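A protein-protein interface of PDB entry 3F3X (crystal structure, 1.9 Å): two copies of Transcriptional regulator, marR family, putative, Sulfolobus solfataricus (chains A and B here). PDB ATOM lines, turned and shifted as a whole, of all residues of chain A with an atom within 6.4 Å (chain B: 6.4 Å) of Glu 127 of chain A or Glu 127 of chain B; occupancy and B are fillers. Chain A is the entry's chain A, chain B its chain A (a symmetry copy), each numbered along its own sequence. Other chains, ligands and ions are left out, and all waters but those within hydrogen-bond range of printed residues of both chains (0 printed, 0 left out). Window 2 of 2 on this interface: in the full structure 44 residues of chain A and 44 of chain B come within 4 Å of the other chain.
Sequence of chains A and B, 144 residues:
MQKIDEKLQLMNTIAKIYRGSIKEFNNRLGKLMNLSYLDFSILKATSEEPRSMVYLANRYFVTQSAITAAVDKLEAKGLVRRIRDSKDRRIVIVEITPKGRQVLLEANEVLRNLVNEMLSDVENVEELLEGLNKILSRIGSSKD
Glu 127 of chain A touches Glu 127 of chain B (OE1 to OE1, 3.96 Å). Leu 128 of chain A touches Leu 128 of chain B.
Hydrophobic or aromatic side chains of chain A that line the printed part of chain B: Leu 128. Along chain A the printed residues that touch a printed residue of chain B span positions 127 to 128. Among the printed residues, 2 pairs touch across the chains.
Glu 127 of chain A touches its own counterpart, Glu 127 of chain B. Leu 128 of chain B touches its own counterpart, Leu 128 of chain A.
Asn 124 of chain A touches none of the printed residues of chain B. Of chain B, only Glu 127 (3.96 Å) comes within 4 Å of Glu 127 of chain A. Printed residues of chain B within 4 Å of Leu 128 of chain A: Leu 128. Glu 127 of chain B touches one residue of chain A. Of the printed residues of chain A, Leu 128 of chain B touches Leu 128. Glu 130 of chain B touches none of the printed residues of chain A. The nearest residue of chain A that does not touch Glu 127 of chain B is Leu 128 of chain A (4.2 Å). The nearest printed residue of chain A that does not touch Leu 128 of chain B is Gly 131 of chain A (4.01 Å).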
ATOM      1  N   ASN A 124     -19.592   7.769  22.493  1.00  0.00           N
ATOM      2  CA  ASN A 124     -18.840   6.640  23.042  1.00  0.00           C
ATOM      3  C   ASN A 124     -17.707   7.126  23.941  1.00  0.00           C
ATOM      4  O   ASN A 124     -16.594   6.597  23.903  1.00  0.00           O
ATOM      5  CB  ASN A 124     -18.258   5.783  21.914  1.00  0.00           C
ATOM      6  CG  ASN A 124     -19.331   5.205  21.004  1.00  0.00           C
ATOM      7  OD1 ASN A 124     -20.220   4.471  21.450  1.00  0.00           O
ATOM      8  ND2 ASN A 124     -19.252   5.533  19.718  1.00  0.00           N
ATOM      9  N   VAL A 125     -18.000   8.132  24.756  1.00  0.00           N
ATOM     10  CA  VAL A 125     -17.004   8.690  25.664  1.00  0.00           C
ATOM     11  C   VAL A 125     -16.574   7.685  26.733  1.00  0.00           C
ATOM     12  O   VAL A 125     -15.385   7.510  26.996  1.00  0.00           O
ATOM     13  CB  VAL A 125     -17.547   9.951  26.363  1.00  0.00           C
ATOM     14  CG1 VAL A 125     -16.519  10.484  27.357  1.00  0.00           C
ATOM     15  CG2 VAL A 125     -17.876  11.017  25.327  1.00  0.00           C
ATOM     16  N   GLU A 126     -17.556   7.030  27.345  1.00  0.00           N
ATOM     17  CA  GLU A 126     -17.291   6.054  28.397  1.00  0.00           C
ATOM     18  C   GLU A 126     -16.330   4.961  27.936  1.00  0.00           C
ATOM     19  O   GLU A 126     -15.372   4.626  28.641  1.00  0.00           O
ATOM     20  CB  GLU A 126     -18.609   5.436  28.875  1.00  0.00           C
ATOM     21  CG  GLU A 126     -18.555   4.729  30.231  1.00  0.00           C
ATOM     22  CD  GLU A 126     -17.724   3.469  30.194  1.00  0.00           C
ATOM     23  OE1 GLU A 126     -17.789   2.758  29.166  1.00  0.00           O
ATOM     24  OE2 GLU A 126     -17.022   3.182  31.187  1.00  0.00           O
ATOM     25  N   GLU A 127     -16.583   4.401  26.757  1.00  0.00           N
ATOM     26  CA  GLU A 127     -15.720   3.357  26.218  1.00  0.00           C
ATOM     27  C   GLU A 127     -14.321   3.899  25.932  1.00  0.00           C
ATOM     28  O   GLU A 127     -13.327   3.216  26.170  1.00  0.00           O
ATOM     29  CB  GLU A 127     -16.326   2.776  24.938  1.00  0.00           C
ATOM     30  CG  GLU A 127     -17.620   2.015  25.181  1.00  0.00           C
ATOM     31  CD  GLU A 127     -18.265   1.500  23.908  1.00  0.00           C
ATOM     32  OE1 GLU A 127     -17.637   1.581  22.822  1.00  0.00           O
ATOM     33  OE2 GLU A 127     -19.410   0.996  23.993  1.00  0.00           O
ATOM     34  N   LEU A 128     -14.244   5.122  25.416  1.00  0.00           N
ATOM     35  CA  LEU A 128     -12.951   5.733  25.121  1.00  0.00           C
ATOM     36  C   LEU A 128     -12.190   5.937  26.429  1.00  0.00           C
ATOM     37  O   LEU A 128     -10.970   5.760  26.485  1.00  0.00           O
ATOM     38  CB  LEU A 128     -13.137   7.083  24.422  1.00  0.00           C
ATOM     39  CG  LEU A 128     -13.743   7.072  23.016  1.00  0.00           C
ATOM     40  CD1 LEU A 128     -13.909   8.505  22.515  1.00  0.00           C
ATOM     41  CD2 LEU A 128     -12.840   6.278  22.075  1.00  0.00           C
ATOM     42  N   LEU A 129     -12.924   6.304  27.478  1.00  0.00           N
ATOM     43  CA  LEU A 129     -12.343   6.540  28.787  1.00  0.00           C
ATOM     44  C   LEU A 129     -11.719   5.268  29.346  1.00  0.00           C
ATOM     45  O   LEU A 129     -10.603   5.304  29.884  1.00  0.00           O
ATOM     46  CB  LEU A 129     -13.413   7.071  29.750  1.00  0.00           C
ATOM     47  CG  LEU A 129     -12.921   7.575  31.105  1.00  0.00           C
ATOM     48  CD1 LEU A 129     -11.823   8.619  30.905  1.00  0.00           C
ATOM     49  CD2 LEU A 129     -14.101   8.170  31.859  1.00  0.00           C
ATOM     50  N   GLU A 130     -12.420   4.144  29.222  1.00  0.00           N
ATOM     51  CA  GLU A 130     -11.884   2.887  29.732  1.00  0.00           C
ATOM     52  C   GLU A 130     -10.642   2.496  28.944  1.00  0.00           C
ATOM     53  O   GLU A 130      -9.645   2.080  29.519  1.00  0.00           O
ATOM     54  CB  GLU A 130     -12.906   1.763  29.610  1.00  0.00           C
ATOM     55  CG  GLU A 130     -14.176   1.967  30.407  1.00  0.00           C
ATOM     56  CD  GLU A 130     -14.953   0.678  30.579  1.00  0.00           C
ATOM     57  OE1 GLU A 130     -16.136   0.755  30.970  1.00  0.00           O
ATOM     58  OE2 GLU A 130     -14.379  -0.407  30.331  1.00  0.00           O
ATOM     59  N   GLY A 131     -10.717   2.621  27.621  1.00  0.00           N
ATOM     60  CA  GLY A 131      -9.576   2.279  26.790  1.00  0.00           C
ATOM     61  C   GLY A 131      -8.358   3.109  27.157  1.00  0.00           C
ATOM     62  O   GLY A 131      -7.258   2.582  27.337  1.00  0.00           O
ATOM     63  N   LEU A 132      -8.553   4.419  27.267  1.00  0.00           N
ATOM     64  CA  LEU A 132      -7.456   5.306  27.622  1.00  0.00           C
ATOM     65  C   LEU A 132      -6.905   5.011  29.017  1.00  0.00           C
ATOM     66  O   LEU A 132      -5.692   5.038  29.218  1.00  0.00           O
ATOM     67  CB  LEU A 132      -7.899   6.768  27.515  1.00  0.00           C
ATOM     68  CG  LEU A 132      -8.179   7.223  26.075  1.00  0.00           C
ATOM     69  CD1 LEU A 132      -8.662   8.664  26.076  1.00  0.00           C
ATOM     70  CD2 LEU A 132      -6.911   7.089  25.234  1.00  0.00           C
ATOM     71  N   ASN B 124      -9.979  -3.393  21.151  1.00  0.00           N
ATOM     72  CA  ASN B 124     -10.799  -2.321  20.587  1.00  0.00           C
ATOM     73  C   ASN B 124      -9.934  -1.142  20.156  1.00  0.00           C
ATOM     74  O   ASN B 124     -10.287   0.019  20.371  1.00  0.00           O
ATOM     75  CB  ASN B 124     -11.834  -1.842  21.609  1.00  0.00           C
ATOM     76  CG  ASN B 124     -12.783  -2.948  22.045  1.00  0.00           C
ATOM     77  OD1 ASN B 124     -13.490  -3.544  21.225  1.00  0.00           O
ATOM     78  ND2 ASN B 124     -12.803  -3.227  23.345  1.00  0.00           N
ATOM     79  N   VAL B 125      -8.799  -1.447  19.537  1.00  0.00           N
ATOM     80  CA  VAL B 125      -7.881  -0.410  19.077  1.00  0.00           C
ATOM     81  C   VAL B 125      -8.491   0.444  17.966  1.00  0.00           C
ATOM     82  O   VAL B 125      -8.416   1.673  17.998  1.00  0.00           O
ATOM     83  CB  VAL B 125      -6.571  -1.032  18.558  1.00  0.00           C
ATOM     84  CG1 VAL B 125      -5.648   0.059  18.020  1.00  0.00           C
ATOM     85  CG2 VAL B 125      -5.879  -1.796  19.678  1.00  0.00           C
ATOM     86  N   GLU B 126      -9.091  -0.220  16.983  1.00  0.00           N
ATOM     87  CA  GLU B 126      -9.702   0.469  15.851  1.00  0.00           C
ATOM     88  C   GLU B 126     -10.729   1.507  16.297  1.00  0.00           C
ATOM     89  O   GLU B 126     -10.721   2.646  15.817  1.00  0.00           O
ATOM     90  CB  GLU B 126     -10.353  -0.553  14.912  1.00  0.00           C
ATOM     91  CG  GLU B 126     -10.655  -0.053  13.498  1.00  0.00           C
ATOM     92  CD  GLU B 126     -11.747   0.990  13.474  1.00  0.00           C
ATOM     93  OE1 GLU B 126     -12.708   0.846  14.262  1.00  0.00           O
ATOM     94  OE2 GLU B 126     -11.653   1.940  12.667  1.00  0.00           O
ATOM     95  N   GLU B 127     -11.614   1.119  17.209  1.00  0.00           N
ATOM     96  CA  GLU B 127     -12.629   2.036  17.712  1.00  0.00           C
ATOM     97  C   GLU B 127     -11.988   3.193  18.476  1.00  0.00           C
ATOM     98  O   GLU B 127     -12.433   4.335  18.367  1.00  0.00           O
ATOM     99  CB  GLU B 127     -13.612   1.293  18.621  1.00  0.00           C
ATOM    100  CG  GLU B 127     -14.458   0.272  17.876  1.00  0.00           C
ATOM    101  CD  GLU B 127     -15.382  -0.521  18.783  1.00  0.00           C
ATOM    102  OE1 GLU B 127     -15.506  -0.181  19.987  1.00  0.00           O
ATOM    103  OE2 GLU B 127     -16.004  -1.488  18.285  1.00  0.00           O
ATOM    104  N   LEU B 128     -10.950   2.900  19.253  1.00  0.00           N
ATOM    105  CA  LEU B 128     -10.261   3.940  20.011  1.00  0.00           C
ATOM    106  C   LEU B 128      -9.607   4.915  19.035  1.00  0.00           C
ATOM    107  O   LEU B 128      -9.586   6.125  19.270  1.00  0.00           O
ATOM    108  CB  LEU B 128      -9.189   3.329  20.918  1.00  0.00           C
ATOM    109  CG  LEU B 128      -9.663   2.440  22.072  1.00  0.00           C
ATOM    110  CD1 LEU B 128      -8.456   1.874  22.816  1.00  0.00           C
ATOM    111  CD2 LEU B 128     -10.541   3.254  23.018  1.00  0.00           C
ATOM    112  N   LEU B 129      -9.082   4.373  17.937  1.00  0.00           N
ATOM    113  CA  LEU B 129      -8.424   5.170  16.918  1.00  0.00           C
ATOM    114  C   LEU B 129      -9.396   6.152  16.277  1.00  0.00           C
ATOM    115  O   LEU B 129      -9.058   7.328  16.080  1.00  0.00           O
ATOM    116  CB  LEU B 129      -7.814   4.256  15.847  1.00  0.00           C
ATOM    117  CG  LEU B 129      -6.901   4.922  14.821  1.00  0.00           C
ATOM    118  CD1 LEU B 129      -5.801   5.709  15.535  1.00  0.00           C
ATOM    119  CD2 LEU B 129      -6.301   3.844  13.931  1.00  0.00           C
ATOM    120  N   GLU B 130     -10.602   5.688  15.955  1.00  0.00           N
ATOM    121  CA  GLU B 130     -11.585   6.572  15.340  1.00  0.00           C
ATOM    122  C   GLU B 130     -11.990   7.660  16.325  1.00  0.00           C
ATOM    123  O   GLU B 130     -12.090   8.823  15.960  1.00  0.00           O
ATOM    124  CB  GLU B 130     -12.836   5.802  14.931  1.00  0.00           C
ATOM    125  CG  GLU B 130     -12.611   4.728  13.889  1.00  0.00           C
ATOM    126  CD  GLU B 130     -13.904   4.292  13.233  1.00  0.00           C
ATOM    127  OE1 GLU B 130     -13.896   3.236  12.566  1.00  0.00           O
ATOM    128  OE2 GLU B 130     -14.921   5.008  13.377  1.00  0.00           O
ATOM    129  N   GLY B 131     -12.236   7.267  17.572  1.00  0.00           N
ATOM    130  CA  GLY B 131     -12.621   8.240  18.580  1.00  0.00           C
ATOM    131  C   GLY B 131     -11.556   9.311  18.747  1.00  0.00           C
ATOM    132  O   GLY B 131     -11.852  10.507  18.756  1.00  0.00           O
ATOM    133  N   LEU B 132     -10.307   8.880  18.884  1.00  0.00           N
ATOM    134  CA  LEU B 132      -9.210   9.821  19.043  1.00  0.00           C
ATOM    135  C   LEU B 132      -9.038  10.718  17.817  1.00  0.00           C
ATOM    136  O   LEU B 132      -8.784  11.913  17.959  1.00  0.00           O
ATOM    137  CB  LEU B 132      -7.909   9.074  19.351  1.00  0.00           C
ATOM    138  CG  LEU B 132      -7.901   8.392  20.727  1.00  0.00           C
ATOM    139  CD1 LEU B 132      -6.597   7.634  20.918  1.00  0.00           C
ATOM    140  CD2 LEU B 132      -8.072   9.440  21.824  1.00  0.00           C
